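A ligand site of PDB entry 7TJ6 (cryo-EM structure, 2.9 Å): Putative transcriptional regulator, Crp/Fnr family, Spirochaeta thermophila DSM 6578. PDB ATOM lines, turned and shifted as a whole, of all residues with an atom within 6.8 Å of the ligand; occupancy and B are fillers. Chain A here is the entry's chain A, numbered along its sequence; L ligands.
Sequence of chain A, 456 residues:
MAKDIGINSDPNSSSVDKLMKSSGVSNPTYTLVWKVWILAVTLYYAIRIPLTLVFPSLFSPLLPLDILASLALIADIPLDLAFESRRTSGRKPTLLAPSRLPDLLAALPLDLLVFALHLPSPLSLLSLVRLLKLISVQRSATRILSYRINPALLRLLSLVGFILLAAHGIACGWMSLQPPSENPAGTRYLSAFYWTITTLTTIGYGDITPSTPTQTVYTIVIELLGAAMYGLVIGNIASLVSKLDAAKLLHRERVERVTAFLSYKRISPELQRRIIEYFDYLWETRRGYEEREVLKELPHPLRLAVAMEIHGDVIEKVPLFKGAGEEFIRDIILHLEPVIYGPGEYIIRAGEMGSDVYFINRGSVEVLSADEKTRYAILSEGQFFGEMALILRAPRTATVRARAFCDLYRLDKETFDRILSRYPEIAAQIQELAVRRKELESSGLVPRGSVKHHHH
CG2 of Val 367 touches O4 of the ligand, at 3.4 Å.
Tyr 376 touches the ligand.
Ala 377 touches the ligand.
CA of Phe 385 touches O6 of the ligand (3.4 Å).
Ala 389 touches the ligand (N to O1, 3.6 Å).
N of Ala 398 touches O3 of the ligand (3.6 Å).
Val 400 touches the ligand.
The guanidinium group of Arg 437 is in salt-bridge range of the side-chain carboxylate of Glu 387, 2.4 Å away.
The backbone carbonyl oxygen (O) of Phe 384 sits at hydrogen-bond distance from the guanidinium group (NH2) of Arg 437 (2.4 Å).
The backbone NH of Val 400 lies within hydrogen-bond range of the backbone carbonyl oxygen of Ile 348 (2.7 Å).
OG1 of Thr 397 sits at hydrogen-bond distance from O3 of the ligand (2.7 Å).
N of Thr 397 lies close to O1 of the ligand (3.4 Å).
NH1 of Arg 437 sits at hydrogen-bond distance from O6 of the ligand (3.2 Å).
The backbone NH (N) of Gly 386 sits at hydrogen-bond distance from an oxygen (O6) of the ligand (3.1 Å).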
ATOM      1  N   ILE A 348      12.691 -30.668  21.025  1.00  0.00           N
ATOM      2  CA  ILE A 348      12.663 -31.015  22.437  1.00  0.00           C
ATOM      3  C   ILE A 348      11.931 -32.336  22.621  1.00  0.00           C
ATOM      4  O   ILE A 348      10.891 -32.576  21.988  1.00  0.00           O
ATOM      5  CB  ILE A 348      11.986 -29.898  23.273  1.00  0.00           C
ATOM      6  CG1 ILE A 348      12.949 -28.718  23.471  1.00  0.00           C
ATOM      7  CG2 ILE A 348      11.496 -30.405  24.619  1.00  0.00           C
ATOM      8  CD1 ILE A 348      12.269 -27.478  23.998  1.00  0.00           C
ATOM      9  N   ARG A 349      12.482 -33.204  23.481  1.00  0.00           N
ATOM     10  CA  ARG A 349      11.865 -34.473  23.837  1.00  0.00           C
ATOM     11  C   ARG A 349      11.251 -34.343  25.230  1.00  0.00           C
ATOM     12  O   ARG A 349      11.683 -33.538  26.047  1.00  0.00           O
ATOM     13  CB  ARG A 349      12.878 -35.610  23.808  1.00  0.00           C
ATOM     14  CG  ARG A 349      13.441 -35.923  22.435  1.00  0.00           C
ATOM     15  CD  ARG A 349      14.494 -37.011  22.524  1.00  0.00           C
ATOM     16  NE  ARG A 349      15.010 -37.406  21.224  1.00  0.00           N
ATOM     17  CZ  ARG A 349      14.516 -38.401  20.486  1.00  0.00           C
ATOM     18  NH1 ARG A 349      13.481 -39.104  20.912  1.00  0.00           N
ATOM     19  NH2 ARG A 349      15.076 -38.684  19.322  1.00  0.00           N
ATOM     20  N   GLY A 354      15.655 -30.136  30.849  1.00  0.00           N
ATOM     21  CA  GLY A 354      15.013 -28.961  30.223  1.00  0.00           C
ATOM     22  C   GLY A 354      15.613 -27.655  30.689  1.00  0.00           C
ATOM     23  O   GLY A 354      15.301 -27.218  31.796  1.00  0.00           O
ATOM     24  N   ASP A 356      16.622 -24.848  28.026  1.00  0.00           N
ATOM     25  CA  ASP A 356      16.625 -23.750  27.081  1.00  0.00           C
ATOM     26  C   ASP A 356      15.202 -23.402  26.685  1.00  0.00           C
ATOM     27  O   ASP A 356      14.278 -24.222  26.779  1.00  0.00           O
ATOM     28  CB  ASP A 356      17.438 -24.118  25.833  1.00  0.00           C
ATOM     29  CG  ASP A 356      18.922 -24.178  26.111  1.00  0.00           C
ATOM     30  OD1 ASP A 356      19.353 -23.668  27.169  1.00  0.00           O
ATOM     31  OD2 ASP A 356      19.667 -24.745  25.288  1.00  0.00           O
ATOM     32  N   VAL A 367       3.983 -29.675  18.644  1.00  0.00           N
ATOM     33  CA  VAL A 367       4.166 -30.231  19.978  1.00  0.00           C
ATOM     34  C   VAL A 367       3.234 -31.425  20.108  1.00  0.00           C
ATOM     35  O   VAL A 367       2.022 -31.321  19.862  1.00  0.00           O
ATOM     36  CB  VAL A 367       3.975 -29.173  21.082  1.00  0.00           C
ATOM     37  CG1 VAL A 367       2.543 -28.666  21.173  1.00  0.00           C
ATOM     38  CG2 VAL A 367       4.432 -29.733  22.424  1.00  0.00           C
ATOM     39  N   TYR A 376      -1.915 -31.768  20.170  1.00  0.00           N
ATOM     40  CA  TYR A 376      -1.886 -30.540  20.965  1.00  0.00           C
ATOM     41  C   TYR A 376      -2.133 -29.323  20.085  1.00  0.00           C
ATOM     42  O   TYR A 376      -3.188 -29.206  19.460  1.00  0.00           O
ATOM     43  CB  TYR A 376      -0.573 -30.399  21.730  1.00  0.00           C
ATOM     44  CG  TYR A 376      -0.461 -31.268  22.969  1.00  0.00           C
ATOM     45  CD1 TYR A 376      -1.112 -30.906  24.144  1.00  0.00           C
ATOM     46  CD2 TYR A 376       0.280 -32.430  22.963  1.00  0.00           C
ATOM     47  CE1 TYR A 376      -1.015 -31.685  25.274  1.00  0.00           C
ATOM     48  CE2 TYR A 376       0.374 -33.223  24.091  1.00  0.00           C
ATOM     49  CZ  TYR A 376      -0.270 -32.837  25.249  1.00  0.00           C
ATOM     50  OH  TYR A 376      -0.181 -33.621  26.375  1.00  0.00           O
ATOM     51  N   ALA A 377      -1.153 -28.412  20.022  1.00  0.00           N
ATOM     52  CA  ALA A 377      -1.284 -27.182  19.279  1.00  0.00           C
ATOM     53  C   ALA A 377      -0.104 -27.065  18.319  1.00  0.00           C
ATOM     54  O   ALA A 377       0.983 -27.572  18.593  1.00  0.00           O
ATOM     55  CB  ALA A 377      -1.339 -25.955  20.202  1.00  0.00           C
ATOM     56  N   ILE A 378      -0.329 -26.409  17.191  1.00  0.00           N
ATOM     57  CA  ILE A 378       0.713 -26.151  16.215  1.00  0.00           C
ATOM     58  C   ILE A 378       1.288 -24.759  16.437  1.00  0.00           C
ATOM     59  O   ILE A 378       0.578 -23.756  16.336  1.00  0.00           O
ATOM     60  CB  ILE A 378       0.190 -26.289  14.774  1.00  0.00           C
ATOM     61  CG1 ILE A 378      -0.356 -27.701  14.541  1.00  0.00           C
ATOM     62  CG2 ILE A 378       1.284 -25.960  13.782  1.00  0.00           C
ATOM     63  CD1 ILE A 378       0.597 -28.795  14.935  1.00  0.00           C
ATOM     64  N   LEU A 379       2.589 -24.695  16.733  1.00  0.00           N
ATOM     65  CA  LEU A 379       3.260 -23.418  16.923  1.00  0.00           C
ATOM     66  C   LEU A 379       3.827 -22.961  15.585  1.00  0.00           C
ATOM     67  O   LEU A 379       4.152 -23.786  14.728  1.00  0.00           O
ATOM     68  CB  LEU A 379       4.365 -23.512  17.975  1.00  0.00           C
ATOM     69  CG  LEU A 379       3.962 -23.240  19.433  1.00  0.00           C
ATOM     70  CD1 LEU A 379       2.767 -24.078  19.890  1.00  0.00           C
ATOM     71  CD2 LEU A 379       5.137 -23.455  20.354  1.00  0.00           C
ATOM     72  N   PHE A 384       6.792 -19.057  20.701  1.00  0.00           N
ATOM     73  CA  PHE A 384       7.886 -19.545  21.525  1.00  0.00           C
ATOM     74  C   PHE A 384       7.404 -20.629  22.485  1.00  0.00           C
ATOM     75  O   PHE A 384       6.245 -20.622  22.918  1.00  0.00           O
ATOM     76  CB  PHE A 384       8.553 -18.351  22.229  1.00  0.00           C
ATOM     77  CG  PHE A 384       7.617 -17.558  23.095  1.00  0.00           C
ATOM     78  CD1 PHE A 384       7.407 -17.888  24.420  1.00  0.00           C
ATOM     79  CD2 PHE A 384       6.932 -16.471  22.565  1.00  0.00           C
ATOM     80  CE1 PHE A 384       6.537 -17.141  25.203  1.00  0.00           C
ATOM     81  CE2 PHE A 384       6.063 -15.737  23.335  1.00  0.00           C
ATOM     82  CZ  PHE A 384       5.862 -16.075  24.652  1.00  0.00           C
ATOM     83  N   PHE A 385       8.305 -21.556  22.803  1.00  0.00           N
ATOM     84  CA  PHE A 385       7.995 -22.677  23.682  1.00  0.00           C
ATOM     85  C   PHE A 385       9.171 -22.972  24.597  1.00  0.00           C
ATOM     86  O   PHE A 385      10.320 -22.607  24.327  1.00  0.00           O
ATOM     87  CB  PHE A 385       7.665 -23.938  22.876  1.00  0.00           C
ATOM     88  CG  PHE A 385       8.774 -24.387  21.955  1.00  0.00           C
ATOM     89  CD1 PHE A 385       9.768 -25.244  22.416  1.00  0.00           C
ATOM     90  CD2 PHE A 385       8.840 -23.949  20.642  1.00  0.00           C
ATOM     91  CE1 PHE A 385      10.787 -25.658  21.590  1.00  0.00           C
ATOM     92  CE2 PHE A 385       9.867 -24.371  19.808  1.00  0.00           C
ATOM     93  CZ  PHE A 385      10.841 -25.225  20.282  1.00  0.00           C
ATOM     94  N   GLY A 386       8.886 -23.658  25.702  1.00  0.00           N
ATOM     95  CA  GLY A 386       9.873 -23.994  26.697  1.00  0.00           C
ATOM     96  C   GLY A 386       9.847 -23.261  28.022  1.00  0.00           C
ATOM     97  O   GLY A 386      10.874 -23.289  28.729  1.00  0.00           O
ATOM     98  N   GLU A 387       8.751 -22.614  28.396  1.00  0.00           N
ATOM     99  CA  GLU A 387       8.801 -21.864  29.646  1.00  0.00           C
ATOM    100  C   GLU A 387       8.436 -22.699  30.870  1.00  0.00           C
ATOM    101  O   GLU A 387       8.964 -22.454  31.950  1.00  0.00           O
ATOM    102  CB  GLU A 387       7.856 -20.664  29.557  1.00  0.00           C
ATOM    103  CG  GLU A 387       8.164 -19.641  28.485  1.00  0.00           C
ATOM    104  CD  GLU A 387       7.663 -20.084  27.141  1.00  0.00           C
ATOM    105  OE1 GLU A 387       6.424 -20.074  26.964  1.00  0.00           O
ATOM    106  OE2 GLU A 387       8.484 -20.415  26.259  1.00  0.00           O
ATOM    107  N   MET A 388       7.572 -23.710  30.703  1.00  0.00           N
ATOM    108  CA  MET A 388       7.101 -24.514  31.819  1.00  0.00           C
ATOM    109  C   MET A 388       8.252 -25.240  32.530  1.00  0.00           C
ATOM    110  O   MET A 388       8.312 -25.238  33.765  1.00  0.00           O
ATOM    111  CB  MET A 388       6.000 -25.469  31.338  1.00  0.00           C
ATOM    112  CG  MET A 388       4.752 -24.652  30.963  1.00  0.00           C
ATOM    113  SD  MET A 388       3.286 -25.441  30.274  1.00  0.00           S
ATOM    114  CE  MET A 388       2.619 -26.292  31.683  1.00  0.00           C
ATOM    115  N   ALA A 389       9.140 -25.806  31.746  1.00  0.00           N
ATOM    116  CA  ALA A 389      10.290 -26.479  32.363  1.00  0.00           C
ATOM    117  C   ALA A 389      10.936 -25.603  33.439  1.00  0.00           C
ATOM    118  O   ALA A 389      11.415 -26.172  34.420  1.00  0.00           O
ATOM    119  CB  ALA A 389      11.279 -26.864  31.297  1.00  0.00           C
ATOM    120  N   LEU A 390      10.984 -24.287  33.247  1.00  0.00           N
ATOM    121  CA  LEU A 390      11.724 -23.447  34.219  1.00  0.00           C
ATOM    122  C   LEU A 390      10.805 -22.539  35.035  1.00  0.00           C
ATOM    123  O   LEU A 390      11.253 -22.109  36.105  1.00  0.00           O
ATOM    124  CB  LEU A 390      12.802 -22.652  33.503  1.00  0.00           C
ATOM    125  CG  LEU A 390      14.214 -23.238  33.637  1.00  0.00           C
ATOM    126  CD1 LEU A 390      15.231 -22.378  32.889  1.00  0.00           C
ATOM    127  CD2 LEU A 390      14.600 -23.372  35.099  1.00  0.00           C
ATOM    128  N   ALA A 394      10.135 -28.946  36.283  1.00  0.00           N
ATOM    129  CA  ALA A 394       9.705 -30.318  35.994  1.00  0.00           C
ATOM    130  C   ALA A 394      10.503 -30.907  34.844  1.00  0.00           C
ATOM    131  O   ALA A 394      11.300 -30.157  34.277  1.00  0.00           O
ATOM    132  CB  ALA A 394       8.230 -30.292  35.684  1.00  0.00           C
ATOM    133  N   PRO A 395      10.374 -32.205  34.458  1.00  0.00           N
ATOM    134  CA  PRO A 395      11.164 -32.647  33.326  1.00  0.00           C
ATOM    135  C   PRO A 395      10.345 -32.212  32.115  1.00  0.00           C
ATOM    136  O   PRO A 395       9.210 -31.819  32.303  1.00  0.00           O
ATOM    137  CB  PRO A 395      11.171 -34.169  33.473  1.00  0.00           C
ATOM    138  CG  PRO A 395       9.882 -34.469  34.199  1.00  0.00           C
ATOM    139  CD  PRO A 395       9.713 -33.309  35.156  1.00  0.00           C
ATOM    140  N   ARG A 396      10.895 -32.313  30.904  1.00  0.00           N
ATOM    141  CA  ARG A 396      10.186 -31.735  29.729  1.00  0.00           C
ATOM    142  C   ARG A 396       8.758 -32.280  29.617  1.00  0.00           C
ATOM    143  O   ARG A 396       8.588 -33.511  29.665  1.00  0.00           O
ATOM    144  CB  ARG A 396      11.002 -31.936  28.450  1.00  0.00           C
ATOM    145  CG  ARG A 396      12.301 -31.152  28.404  1.00  0.00           C
ATOM    146  CD  ARG A 396      13.046 -31.337  27.096  1.00  0.00           C
ATOM    147  NE  ARG A 396      14.316 -30.626  27.120  1.00  0.00           N
ATOM    148  CZ  ARG A 396      15.241 -30.697  26.169  1.00  0.00           C
ATOM    149  NH1 ARG A 396      15.032 -31.456  25.112  1.00  0.00           N
ATOM    150  NH2 ARG A 396      16.354 -29.998  26.278  1.00  0.00           N
ATOM    151  N   THR A 397       7.787 -31.374  29.474  1.00  0.00           N
ATOM    152  CA  THR A 397       6.360 -31.767  29.461  1.00  0.00           C
ATOM    153  C   THR A 397       5.957 -32.541  28.222  1.00  0.00           C
ATOM    154  O   THR A 397       5.236 -33.542  28.379  1.00  0.00           O
ATOM    155  CB  THR A 397       5.499 -30.530  29.628  1.00  0.00           C
ATOM    156  OG1 THR A 397       5.626 -29.745  28.441  1.00  0.00           O
ATOM    157  CG2 THR A 397       5.922 -29.727  30.844  1.00  0.00           C
ATOM    158  N   ALA A 398       6.385 -32.122  27.040  1.00  0.00           N
ATOM    159  CA  ALA A 398       5.915 -32.792  25.813  1.00  0.00           C
ATOM    160  C   ALA A 398       7.022 -32.796  24.759  1.00  0.00           C
ATOM    161  O   ALA A 398       8.096 -32.228  25.038  1.00  0.00           O
ATOM    162  CB  ALA A 398       4.675 -32.090  25.324  1.00  0.00           C
ATOM    163  N   THR A 399       6.771 -33.409  23.608  1.00  0.00           N
ATOM    164  CA  THR A 399       7.791 -33.467  22.568  1.00  0.00           C
ATOM    165  C   THR A 399       7.491 -32.471  21.464  1.00  0.00           C
ATOM    166  O   THR A 399       6.343 -32.314  21.041  1.00  0.00           O
ATOM    167  CB  THR A 399       7.861 -34.878  21.954  1.00  0.00           C
ATOM    168  OG1 THR A 399       6.587 -35.228  21.399  1.00  0.00           O
ATOM    169  CG2 THR A 399       8.219 -35.895  23.015  1.00  0.00           C
ATOM    170  N   VAL A 400       8.530 -31.784  20.996  1.00  0.00           N
ATOM    171  CA  VAL A 400       8.394 -30.786  19.941  1.00  0.00           C
ATOM    172  C   VAL A 400       9.125 -31.298  18.702  1.00  0.00           C
ATOM    173  O   VAL A 400      10.333 -31.550  18.741  1.00  0.00           O
ATOM    174  CB  VAL A 400       8.962 -29.423  20.376  1.00  0.00           C
ATOM    175  CG1 VAL A 400       8.775 -28.402  19.268  1.00  0.00           C
ATOM    176  CG2 VAL A 400       8.291 -28.963  21.658  1.00  0.00           C
ATOM    177  N   ARG A 436      -1.727 -21.187  31.216  1.00  0.00           N
ATOM    178  CA  ARG A 436      -2.720 -21.521  30.172  1.00  0.00           C
ATOM    179  C   ARG A 436      -2.224 -22.751  29.436  1.00  0.00           C
ATOM    180  O   ARG A 436      -3.058 -23.569  29.013  1.00  0.00           O
ATOM    181  CB  ARG A 436      -2.867 -20.357  29.199  1.00  0.00           C
ATOM    182  CG  ARG A 436      -3.842 -19.283  29.655  1.00  0.00           C
ATOM    183  CD  ARG A 436      -3.408 -17.891  29.240  1.00  0.00           C
ATOM    184  NE  ARG A 436      -2.972 -17.816  27.863  1.00  0.00           N
ATOM    185  CZ  ARG A 436      -2.425 -16.751  27.299  1.00  0.00           C
ATOM    186  NH1 ARG A 436      -2.060 -16.775  26.037  1.00  0.00           N
ATOM    187  NH2 ARG A 436      -2.235 -15.655  28.023  1.00  0.00           N
ATOM    188  N   ARG A 437      -0.914 -22.892  29.330  1.00  0.00           N
ATOM    189  CA  ARG A 437      -0.329 -23.971  28.534  1.00  0.00           C
ATOM    190  C   ARG A 437      -0.410 -25.288  29.279  1.00  0.00           C
ATOM    191  O   ARG A 437      -0.707 -25.330  30.478  1.00  0.00           O
ATOM    192  CB  ARG A 437       1.112 -23.653  28.156  1.00  0.00           C
ATOM    193  CG  ARG A 437       1.225 -22.965  26.826  1.00  0.00           C
ATOM    194  CD  ARG A 437       2.616 -22.445  26.594  1.00  0.00           C
ATOM    195  NE  ARG A 437       2.799 -22.083  25.205  1.00  0.00           N
ATOM    196  CZ  ARG A 437       3.907 -21.534  24.713  1.00  0.00           C
ATOM    197  NH1 ARG A 437       4.950 -21.305  25.488  1.00  0.00           N
ATOM    198  NH2 ARG A 437       3.973 -21.263  23.421  1.00  0.00           N
HETATM  199  P1  LIG L   1       8.204 -27.595  27.597  1.00  0.00           P
HETATM  200  O1  LIG L   1       8.160 -28.025  29.040  1.00  0.00           O
HETATM  201  O2  LIG L   1       9.531 -27.310  26.940  1.00  0.00           O
HETATM  202  O3  LIG L   1       7.439 -28.697  26.715  1.00  0.00           O
HETATM  203  C1  LIG L   1       7.211 -28.446  25.329  1.00  0.00           C
HETATM  204  C2  LIG L   1       6.489 -27.139  25.245  1.00  0.00           C
HETATM  205  O4  LIG L   1       5.211 -27.212  24.587  1.00  0.00           O
HETATM  206  C3  LIG L   1       6.111 -26.619  26.601  1.00  0.00           C
HETATM  207  O5  LIG L   1       7.259 -26.290  27.374  1.00  0.00           O
HETATM  208  C4  LIG L   1       5.138 -25.506  26.254  1.00  0.00           C
HETATM  209  O6  LIG L   1       5.842 -24.357  25.785  1.00  0.00           O
HETATM  210  C5  LIG L   1       4.409 -26.147  25.061  1.00  0.00           C
HETATM  211  N1  LIG L   1       3.074 -26.674  25.425  1.00  0.00           N
HETATM  212  C6  LIG L   1       2.819 -27.597  26.363  1.00  0.00           C
HETATM  213  N2  LIG L   1       1.485 -27.860  26.442  1.00  0.00           N
HETATM  214  C7  LIG L   1       0.869 -27.079  25.537  1.00  0.00           C
HETATM  215  C8  LIG L   1      -0.529 -26.849  25.101  1.00  0.00           C
HETATM  216  N3  LIG L   1      -1.555 -27.527  25.662  1.00  0.00           N
HETATM  217  N4  LIG L   1      -0.740 -25.948  24.115  1.00  0.00           N
HETATM  218  C9  LIG L   1       0.273 -25.267  23.549  1.00  0.00           C
HETATM  219  N5  LIG L   1       1.559 -25.431  23.899  1.00  0.00           N
HETATM  220  C10 LIG L   1       1.924 -26.300  24.865  1.00  0.00           C
